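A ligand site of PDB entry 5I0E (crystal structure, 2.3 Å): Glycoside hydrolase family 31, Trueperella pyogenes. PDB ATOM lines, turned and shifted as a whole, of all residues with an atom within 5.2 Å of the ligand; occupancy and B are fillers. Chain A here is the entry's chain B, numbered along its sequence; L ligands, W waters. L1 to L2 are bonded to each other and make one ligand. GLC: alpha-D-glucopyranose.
NE2 of His 591 is in hydrogen-bond range of O4 of GLC L1.
The side-chain carboxylate of Glu 335 is in hydrogen-bond range of an oxygen (O6) of GLC L2, at 2.6 Å.
OE1 of Glu 330 lies within hydrogen-bond range of O4 of GLC L1, at 2.6 Å.
NH1 of Arg 516 is in hydrogen-bond range of O2 of GLC L1 (2.9 Å).
O3 of GLC L1 lies within hydrogen-bond range of NZ of Lys 465 (3.2 Å).
An oxygen (O5) of GLC L2 lies within hydrogen-bond range of the side-chain amide nitrogen (ND2) of Asn 302 (2.9 Å).
OD1 of Asp 532 is in hydrogen-bond range of O2 of GLC L1 (2.6 Å).
The guanidinium group (NH2) of Arg 516 is in salt-bridge range of the side-chain carboxylate (OE2) of Glu 198 (3.2 Å).
The indole nitrogen (NE1) of Trp 387 is in hydrogen-bond range of the side-chain carboxylate (OD2) of Asp 467 (2.8 Å).
The backbone carbonyl oxygen of Phe 565 lies within hydrogen-bond range of the backbone NH of Glu 593, 2.9 Å away.
The backbone carbonyl oxygen (O) of Glu 335 sits at hydrogen-bond distance from the side-chain amino group (NZ) of Lys 393 (2.8 Å).
NE of Arg 516 lies within salt-bridge range of OD1 of Asp 467 (3.3 Å).
The side-chain carboxylate (OD2) of Asp 532 is in salt-bridge range of the guanidinium group (NH1) of Arg 516 (3.7 Å).
NZ of Lys 465 lies within salt-bridge range of OE2 of Glu 330, 2.7 Å away.
NE2 of His 591 lies within hydrogen-bond range of OE2 of Glu 330, 3.3 Å away.
The side-chain carboxylate of Asp 467 sits close to an oxygen (O5) of GLC L1.
Merely in contact with the ligand: Trp 430, Ala 331, Trp 529, Phe 338, Phe 565 and Trp 387.
Hydrophobic or aromatic side chains that line the ligand: Ala 331, Phe 338, Trp 387, Trp 430, Trp 529, Phe 565 and His 591.
Of the 22 residues printed, 14 come within 4 Å of the ligand.
Water W2 bridges O6 of GLC L2 (2.7 Å) and OD1 of Asn 302 (2.8 Å).
Water W1 lies within hydrogen-bond range of an oxygen (O3) of GLC L2 (2.7 Å) and the side-chain amino group (NZ) of Lys 393 (2.9 Å).
Water W5 bridges an oxygen (O4) of GLC L1 (2.8 Å) and the backbone NH of Phe 594 (2.8 Å).
Water W4 lies within hydrogen-bond range of OE2 of Glu 198 (2.7 Å), O1 of GLC L1 (3.4 Å) and NH2 of Arg 516 (3.5 Å).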
ATOM      1  N   GLU A 198      -8.926   6.390 -34.253  1.00  0.00           N
ATOM      2  CA  GLU A 198      -7.820   7.209 -33.739  1.00  0.00           C
ATOM      3  C   GLU A 198      -6.601   6.316 -33.497  1.00  0.00           C
ATOM      4  O   GLU A 198      -6.562   5.579 -32.503  1.00  0.00           O
ATOM      5  CB  GLU A 198      -8.171   7.968 -32.448  1.00  0.00           C
ATOM      6  CG  GLU A 198      -6.946   8.677 -31.883  1.00  0.00           C
ATOM      7  CD  GLU A 198      -7.183   9.463 -30.625  1.00  0.00           C
ATOM      8  OE1 GLU A 198      -8.193   9.204 -29.943  1.00  0.00           O
ATOM      9  OE2 GLU A 198      -6.326  10.323 -30.317  1.00  0.00           O
ATOM     10  N   ASN A 302      -0.234  23.808 -27.552  1.00  0.00           N
ATOM     11  CA  ASN A 302      -1.184  23.439 -26.495  1.00  0.00           C
ATOM     12  C   ASN A 302      -0.953  24.172 -25.162  1.00  0.00           C
ATOM     13  O   ASN A 302      -1.874  24.373 -24.405  1.00  0.00           O
ATOM     14  CB  ASN A 302      -1.227  21.932 -26.272  1.00  0.00           C
ATOM     15  CG  ASN A 302      -2.389  21.517 -25.379  1.00  0.00           C
ATOM     16  OD1 ASN A 302      -2.216  21.373 -24.185  1.00  0.00           O
ATOM     17  ND2 ASN A 302      -3.584  21.425 -25.946  1.00  0.00           N
ATOM     18  N   GLU A 330      -5.993  26.025 -27.912  1.00  0.00           N
ATOM     19  CA  GLU A 330      -6.576  24.738 -27.498  1.00  0.00           C
ATOM     20  C   GLU A 330      -6.991  24.789 -26.044  1.00  0.00           C
ATOM     21  O   GLU A 330      -8.137  24.508 -25.721  1.00  0.00           O
ATOM     22  CB  GLU A 330      -5.608  23.583 -27.774  1.00  0.00           C
ATOM     23  CG  GLU A 330      -5.386  23.372 -29.267  1.00  0.00           C
ATOM     24  CD  GLU A 330      -4.704  22.048 -29.579  1.00  0.00           C
ATOM     25  OE1 GLU A 330      -3.945  21.548 -28.719  1.00  0.00           O
ATOM     26  OE2 GLU A 330      -4.908  21.515 -30.676  1.00  0.00           O
ATOM     27  N   ALA A 331      -6.057  25.171 -25.184  1.00  0.00           N
ATOM     28  CA  ALA A 331      -6.307  25.237 -23.745  1.00  0.00           C
ATOM     29  C   ALA A 331      -6.840  26.631 -23.391  1.00  0.00           C
ATOM     30  O   ALA A 331      -6.134  27.433 -22.765  1.00  0.00           O
ATOM     31  CB  ALA A 331      -5.037  24.917 -23.009  1.00  0.00           C
ATOM     32  N   GLU A 335     -11.830  23.523 -19.142  1.00  0.00           N
ATOM     33  CA  GLU A 335     -11.435  22.098 -19.193  1.00  0.00           C
ATOM     34  C   GLU A 335     -12.495  21.137 -18.608  1.00  0.00           C
ATOM     35  O   GLU A 335     -12.192  19.991 -18.260  1.00  0.00           O
ATOM     36  CB  GLU A 335     -10.055  21.901 -18.516  1.00  0.00           C
ATOM     37  CG  GLU A 335      -8.902  22.610 -19.244  1.00  0.00           C
ATOM     38  CD  GLU A 335      -8.673  22.089 -20.675  1.00  0.00           C
ATOM     39  OE1 GLU A 335      -8.903  20.885 -20.940  1.00  0.00           O
ATOM     40  OE2 GLU A 335      -8.252  22.880 -21.552  1.00  0.00           O
ATOM     41  N   PHE A 338     -15.920  23.014 -22.135  1.00  0.00           N
ATOM     42  CA  PHE A 338     -15.427  23.527 -23.419  1.00  0.00           C
ATOM     43  C   PHE A 338     -16.339  24.541 -24.118  1.00  0.00           C
ATOM     44  O   PHE A 338     -16.436  24.607 -25.353  1.00  0.00           O
ATOM     45  CB  PHE A 338     -15.034  22.361 -24.317  1.00  0.00           C
ATOM     46  CG  PHE A 338     -14.010  21.473 -23.648  1.00  0.00           C
ATOM     47  CD1 PHE A 338     -12.668  21.852 -23.627  1.00  0.00           C
ATOM     48  CD2 PHE A 338     -14.391  20.311 -22.976  1.00  0.00           C
ATOM     49  CE1 PHE A 338     -11.726  21.079 -22.970  1.00  0.00           C
ATOM     50  CE2 PHE A 338     -13.463  19.536 -22.321  1.00  0.00           C
ATOM     51  CZ  PHE A 338     -12.119  19.915 -22.316  1.00  0.00           C
ATOM     52  N   TRP A 387     -10.361  25.219 -29.963  1.00  0.00           N
ATOM     53  CA  TRP A 387     -10.443  23.763 -30.028  1.00  0.00           C
ATOM     54  C   TRP A 387     -11.778  23.316 -29.458  1.00  0.00           C
ATOM     55  O   TRP A 387     -12.346  23.966 -28.572  1.00  0.00           O
ATOM     56  CB  TRP A 387      -9.280  23.198 -29.201  1.00  0.00           C
ATOM     57  CG  TRP A 387      -9.100  21.737 -29.102  1.00  0.00           C
ATOM     58  CD1 TRP A 387      -8.286  20.973 -29.889  1.00  0.00           C
ATOM     59  CD2 TRP A 387      -9.645  20.871 -28.114  1.00  0.00           C
ATOM     60  NE1 TRP A 387      -8.326  19.671 -29.480  1.00  0.00           N
ATOM     61  CE2 TRP A 387      -9.139  19.579 -28.376  1.00  0.00           C
ATOM     62  CE3 TRP A 387     -10.508  21.065 -27.036  1.00  0.00           C
ATOM     63  CZ2 TRP A 387      -9.480  18.455 -27.605  1.00  0.00           C
ATOM     64  CZ3 TRP A 387     -10.860  19.969 -26.272  1.00  0.00           C
ATOM     65  CH2 TRP A 387     -10.342  18.658 -26.556  1.00  0.00           C
ATOM     66  N   LYS A 393     -17.820  15.593 -20.932  1.00  0.00           N
ATOM     67  CA  LYS A 393     -17.240  14.903 -19.755  1.00  0.00           C
ATOM     68  C   LYS A 393     -18.311  14.646 -18.685  1.00  0.00           C
ATOM     69  O   LYS A 393     -19.238  15.445 -18.514  1.00  0.00           O
ATOM     70  CB  LYS A 393     -16.100  15.702 -19.133  1.00  0.00           C
ATOM     71  CG  LYS A 393     -14.796  15.774 -19.909  1.00  0.00           C
ATOM     72  CD  LYS A 393     -13.760  16.562 -19.119  1.00  0.00           C
ATOM     73  CE  LYS A 393     -12.378  16.479 -19.729  1.00  0.00           C
ATOM     74  NZ  LYS A 393     -11.440  17.502 -19.169  1.00  0.00           N
ATOM     75  N   TRP A 430      -9.109   7.963 -23.085  1.00  0.00           N
ATOM     76  CA  TRP A 430      -9.154   9.442 -23.197  1.00  0.00           C
ATOM     77  C   TRP A 430     -10.614   9.864 -23.004  1.00  0.00           C
ATOM     78  O   TRP A 430     -11.491   9.392 -23.738  1.00  0.00           O
ATOM     79  CB  TRP A 430      -8.610   9.854 -24.600  1.00  0.00           C
ATOM     80  CG  TRP A 430      -8.755  11.317 -25.136  1.00  0.00           C
ATOM     81  CD1 TRP A 430      -9.936  12.010 -25.421  1.00  0.00           C
ATOM     82  CD2 TRP A 430      -7.682  12.200 -25.541  1.00  0.00           C
ATOM     83  NE1 TRP A 430      -9.640  13.268 -25.925  1.00  0.00           N
ATOM     84  CE2 TRP A 430      -8.277  13.412 -26.007  1.00  0.00           C
ATOM     85  CE3 TRP A 430      -6.273  12.085 -25.533  1.00  0.00           C
ATOM     86  CZ2 TRP A 430      -7.507  14.502 -26.452  1.00  0.00           C
ATOM     87  CZ3 TRP A 430      -5.503  13.176 -25.978  1.00  0.00           C
ATOM     88  CH2 TRP A 430      -6.133  14.369 -26.431  1.00  0.00           C
ATOM     89  N   PHE A 431     -10.892  10.738 -22.015  1.00  0.00           N
ATOM     90  CA  PHE A 431     -12.260  11.215 -21.694  1.00  0.00           C
ATOM     91  C   PHE A 431     -13.175  10.008 -21.396  1.00  0.00           C
ATOM     92  O   PHE A 431     -14.174   9.784 -22.096  1.00  0.00           O
ATOM     93  CB  PHE A 431     -12.894  12.073 -22.825  1.00  0.00           C
ATOM     94  CG  PHE A 431     -12.409  13.501 -22.897  1.00  0.00           C
ATOM     95  CD1 PHE A 431     -11.100  13.856 -22.682  1.00  0.00           C
ATOM     96  CD2 PHE A 431     -13.298  14.507 -23.285  1.00  0.00           C
ATOM     97  CE1 PHE A 431     -10.677  15.167 -22.804  1.00  0.00           C
ATOM     98  CE2 PHE A 431     -12.892  15.832 -23.398  1.00  0.00           C
ATOM     99  CZ  PHE A 431     -11.572  16.159 -23.177  1.00  0.00           C
ATOM    100  N   LYS A 465     -11.186  24.445 -34.130  1.00  0.00           N
ATOM    101  CA  LYS A 465     -10.457  23.217 -34.353  1.00  0.00           C
ATOM    102  C   LYS A 465     -11.351  22.069 -33.819  1.00  0.00           C
ATOM    103  O   LYS A 465     -11.333  21.726 -32.630  1.00  0.00           O
ATOM    104  CB  LYS A 465      -9.057  23.272 -33.701  1.00  0.00           C
ATOM    105  CG  LYS A 465      -8.266  22.000 -33.843  1.00  0.00           C
ATOM    106  CD  LYS A 465      -6.810  22.177 -33.408  1.00  0.00           C
ATOM    107  CE  LYS A 465      -6.029  20.906 -33.708  1.00  0.00           C
ATOM    108  NZ  LYS A 465      -4.599  20.914 -33.310  1.00  0.00           N
ATOM    109  N   ASP A 467     -11.701  18.791 -33.276  1.00  0.00           N
ATOM    110  CA  ASP A 467     -10.841  17.642 -33.064  1.00  0.00           C
ATOM    111  C   ASP A 467     -11.706  16.463 -32.667  1.00  0.00           C
ATOM    112  O   ASP A 467     -12.856  16.664 -32.295  1.00  0.00           O
ATOM    113  CB  ASP A 467      -9.869  18.014 -31.957  1.00  0.00           C
ATOM    114  CG  ASP A 467      -8.853  16.960 -31.666  1.00  0.00           C
ATOM    115  OD1 ASP A 467      -8.482  16.125 -32.521  1.00  0.00           O
ATOM    116  OD2 ASP A 467      -8.385  17.026 -30.519  1.00  0.00           O
ATOM    117  N   ARG A 516      -9.520  16.485 -37.985  1.00  0.00           N
ATOM    118  CA  ARG A 516      -8.618  15.391 -38.330  1.00  0.00           C
ATOM    119  C   ARG A 516      -9.335  14.151 -38.813  1.00  0.00           C
ATOM    120  O   ARG A 516      -8.756  13.381 -39.568  1.00  0.00           O
ATOM    121  CB  ARG A 516      -7.688  15.048 -37.179  1.00  0.00           C
ATOM    122  CG  ARG A 516      -8.305  14.174 -36.117  1.00  0.00           C
ATOM    123  CD  ARG A 516      -7.443  14.018 -34.881  1.00  0.00           C
ATOM    124  NE  ARG A 516      -8.152  13.209 -33.921  1.00  0.00           N
ATOM    125  CZ  ARG A 516      -7.714  12.881 -32.714  1.00  0.00           C
ATOM    126  NH1 ARG A 516      -6.516  13.277 -32.283  1.00  0.00           N
ATOM    127  NH2 ARG A 516      -8.473  12.148 -31.926  1.00  0.00           N
ATOM    128  N   TRP A 529      -6.329  18.451 -41.051  1.00  0.00           N
ATOM    129  CA  TRP A 529      -4.896  18.246 -40.758  1.00  0.00           C
ATOM    130  C   TRP A 529      -4.652  16.773 -40.502  1.00  0.00           C
ATOM    131  O   TRP A 529      -5.579  16.051 -40.145  1.00  0.00           O
ATOM    132  CB  TRP A 529      -4.372  19.132 -39.604  1.00  0.00           C
ATOM    133  CG  TRP A 529      -4.383  18.571 -38.180  1.00  0.00           C
ATOM    134  CD1 TRP A 529      -3.309  18.080 -37.500  1.00  0.00           C
ATOM    135  CD2 TRP A 529      -5.483  18.518 -37.258  1.00  0.00           C
ATOM    136  NE1 TRP A 529      -3.674  17.687 -36.233  1.00  0.00           N
ATOM    137  CE2 TRP A 529      -5.009  17.936 -36.072  1.00  0.00           C
ATOM    138  CE3 TRP A 529      -6.833  18.932 -37.327  1.00  0.00           C
ATOM    139  CZ2 TRP A 529      -5.835  17.734 -34.944  1.00  0.00           C
ATOM    140  CZ3 TRP A 529      -7.651  18.728 -36.209  1.00  0.00           C
ATOM    141  CH2 TRP A 529      -7.149  18.130 -35.044  1.00  0.00           C
ATOM    142  N   GLY A 531      -3.221  14.947 -38.189  1.00  0.00           N
ATOM    143  CA  GLY A 531      -3.239  14.402 -36.842  1.00  0.00           C
ATOM    144  C   GLY A 531      -1.902  14.354 -36.125  1.00  0.00           C
ATOM    145  O   GLY A 531      -1.014  15.160 -36.385  1.00  0.00           O
ATOM    146  N   ASP A 532      -1.764  13.382 -35.226  1.00  0.00           N
ATOM    147  CA  ASP A 532      -0.698  13.340 -34.231  1.00  0.00           C
ATOM    148  C   ASP A 532       0.496  12.539 -34.703  1.00  0.00           C
ATOM    149  O   ASP A 532       0.354  11.371 -35.091  1.00  0.00           O
ATOM    150  CB  ASP A 532      -1.227  12.697 -32.938  1.00  0.00           C
ATOM    151  CG  ASP A 532      -2.329  13.519 -32.292  1.00  0.00           C
ATOM    152  OD1 ASP A 532      -2.553  14.679 -32.718  1.00  0.00           O
ATOM    153  OD2 ASP A 532      -2.990  13.012 -31.364  1.00  0.00           O
ATOM    154  N   ASP A 561       1.033  19.074 -38.764  1.00  0.00           N
ATOM    155  CA  ASP A 561       1.877  19.712 -37.733  1.00  0.00           C
ATOM    156  C   ASP A 561       3.310  19.632 -38.226  1.00  0.00           C
ATOM    157  O   ASP A 561       3.955  18.594 -38.116  1.00  0.00           O
ATOM    158  CB  ASP A 561       1.759  18.986 -36.396  1.00  0.00           C
ATOM    159  CG  ASP A 561       0.315  18.931 -35.861  1.00  0.00           C
ATOM    160  OD1 ASP A 561      -0.585  19.667 -36.335  1.00  0.00           O
ATOM    161  OD2 ASP A 561       0.090  18.101 -34.953  1.00  0.00           O
ATOM    162  N   PHE A 565       4.498  17.189 -33.652  1.00  0.00           N
ATOM    163  CA  PHE A 565       4.033  17.922 -32.467  1.00  0.00           C
ATOM    164  C   PHE A 565       4.380  17.255 -31.123  1.00  0.00           C
ATOM    165  O   PHE A 565       4.353  17.942 -30.106  1.00  0.00           O
ATOM    166  CB  PHE A 565       2.531  18.255 -32.595  1.00  0.00           C
ATOM    167  CG  PHE A 565       1.584  17.371 -31.786  1.00  0.00           C
ATOM    168  CD1 PHE A 565       1.614  15.996 -31.870  1.00  0.00           C
ATOM    169  CD2 PHE A 565       0.584  17.956 -31.008  1.00  0.00           C
ATOM    170  CE1 PHE A 565       0.713  15.199 -31.146  1.00  0.00           C
ATOM    171  CE2 PHE A 565      -0.332  17.166 -30.279  1.00  0.00           C
ATOM    172  CZ  PHE A 565      -0.267  15.792 -30.354  1.00  0.00           C
ATOM    173  N   HIS A 591       2.540  23.283 -34.436  1.00  0.00           N
ATOM    174  CA  HIS A 591       1.744  22.933 -33.303  1.00  0.00           C
ATOM    175  C   HIS A 591       2.655  22.127 -32.337  1.00  0.00           C
ATOM    176  O   HIS A 591       3.694  21.585 -32.766  1.00  0.00           O
ATOM    177  CB  HIS A 591       0.565  22.086 -33.768  1.00  0.00           C
ATOM    178  CG  HIS A 591      -0.366  21.689 -32.652  1.00  0.00           C
ATOM    179  ND1 HIS A 591      -0.794  22.576 -31.696  1.00  0.00           N
ATOM    180  CD2 HIS A 591      -0.980  20.515 -32.384  1.00  0.00           C
ATOM    181  CE1 HIS A 591      -1.592  21.952 -30.845  1.00  0.00           C
ATOM    182  NE2 HIS A 591      -1.734  20.701 -31.242  1.00  0.00           N
ATOM    183  N   SER A 592       2.275  22.087 -31.055  1.00  0.00           N
ATOM    184  CA  SER A 592       2.976  21.304 -30.053  1.00  0.00           C
ATOM    185  C   SER A 592       1.995  20.636 -29.119  1.00  0.00           C
ATOM    186  O   SER A 592       0.971  21.202 -28.786  1.00  0.00           O
ATOM    187  CB  SER A 592       3.965  22.182 -29.231  1.00  0.00           C
ATOM    188  OG  SER A 592       3.308  23.289 -28.649  1.00  0.00           O
ATOM    189  N   GLU A 593       2.346  19.435 -28.680  1.00  0.00           N
ATOM    190  CA  GLU A 593       1.524  18.632 -27.750  1.00  0.00           C
ATOM    191  C   GLU A 593       1.659  19.129 -26.319  1.00  0.00           C
ATOM    192  O   GLU A 593       2.701  19.633 -25.932  1.00  0.00           O
ATOM    193  CB  GLU A 593       1.967  17.166 -27.797  1.00  0.00           C
ATOM    194  CG  GLU A 593       1.046  16.189 -27.075  1.00  0.00           C
ATOM    195  CD  GLU A 593       1.398  14.727 -27.330  1.00  0.00           C
ATOM    196  OE1 GLU A 593       2.589  14.361 -27.208  1.00  0.00           O
ATOM    197  OE2 GLU A 593       0.481  13.953 -27.670  1.00  0.00           O
ATOM    198  N   PHE A 594       0.591  18.938 -25.543  1.00  0.00           N
ATOM    199  CA  PHE A 594       0.564  19.132 -24.099  1.00  0.00           C
ATOM    200  C   PHE A 594       1.695  18.356 -23.444  1.00  0.00           C
ATOM    201  O   PHE A 594       1.930  17.215 -23.761  1.00  0.00           O
ATOM    202  CB  PHE A 594      -0.747  18.622 -23.523  1.00  0.00           C
ATOM    203  CG  PHE A 594      -0.908  18.818 -22.041  1.00  0.00           C
ATOM    204  CD1 PHE A 594      -0.970  20.104 -21.486  1.00  0.00           C
ATOM    205  CD2 PHE A 594      -1.065  17.711 -21.197  1.00  0.00           C
ATOM    206  CE1 PHE A 594      -1.159  20.288 -20.118  1.00  0.00           C
ATOM    207  CE2 PHE A 594      -1.268  17.885 -19.819  1.00  0.00           C
ATOM    208  CZ  PHE A 594      -1.308  19.179 -19.285  1.00  0.00           C
HETATM  209  C1  GLC L   1      -5.692  15.807 -29.977  1.00  0.00           C
HETATM  210  C2  GLC L   1      -5.191  16.606 -31.181  1.00  0.00           C
HETATM  211  C3  GLC L   1      -3.963  17.442 -30.804  1.00  0.00           C
HETATM  212  C4  GLC L   1      -4.325  18.358 -29.643  1.00  0.00           C
HETATM  213  C5  GLC L   1      -4.875  17.564 -28.461  1.00  0.00           C
HETATM  214  C6  GLC L   1      -5.387  18.543 -27.402  1.00  0.00           C
HETATM  215  O1  GLC L   1      -4.689  14.854 -29.655  1.00  0.00           O
HETATM  216  O2  GLC L   1      -4.881  15.718 -32.243  1.00  0.00           O
HETATM  217  O3  GLC L   1      -3.566  18.215 -31.939  1.00  0.00           O
HETATM  218  O4  GLC L   1      -3.197  19.144 -29.214  1.00  0.00           O
HETATM  219  O5  GLC L   1      -5.926  16.670 -28.855  1.00  0.00           O
HETATM  220  O6  GLC L   1      -5.708  17.827 -26.198  1.00  0.00           O
HETATM  221  C1  GLC L   2      -5.118  18.447 -25.056  1.00  0.00           C
HETATM  222  C2  GLC L   2      -5.319  17.556 -23.832  1.00  0.00           C
HETATM  223  C3  GLC L   2      -6.794  17.522 -23.440  1.00  0.00           C
HETATM  224  C4  GLC L   2      -7.299  18.948 -23.238  1.00  0.00           C
HETATM  225  C5  GLC L   2      -7.075  19.736 -24.520  1.00  0.00           C
HETATM  226  C6  GLC L   2      -7.502  21.191 -24.419  1.00  0.00           C
HETATM  227  O2  GLC L   2      -4.849  16.225 -24.105  1.00  0.00           O
HETATM  228  O3  GLC L   2      -6.962  16.765 -22.249  1.00  0.00           O
HETATM  229  O4  GLC L   2      -8.680  18.925 -22.864  1.00  0.00           O
HETATM  230  O5  GLC L   2      -5.680  19.726 -24.847  1.00  0.00           O
HETATM  231  O6  GLC L   2      -6.699  21.848 -23.426  1.00  0.00           O
HETATM  232  O   HOH W   1      -8.854  17.147 -20.397  1.00  0.00           O
HETATM  233  O   HOH W   2      -4.337  21.164 -22.399  1.00  0.00           O
HETATM  234  O   HOH W   3      -2.643  15.998 -25.650  1.00  0.00           O
HETATM  235  O   HOH W   4      -6.940  12.513 -28.820  1.00  0.00           O
HETATM  236  O   HOH W   5      -1.917  18.442 -26.791  1.00  0.00           O
HETATM  237  O   HOH W   6      -3.806  14.898 -21.448  1.00  0.00           O
HETATM  238  O   HOH W   7      -2.082  17.149 -33.927  1.00  0.00           O
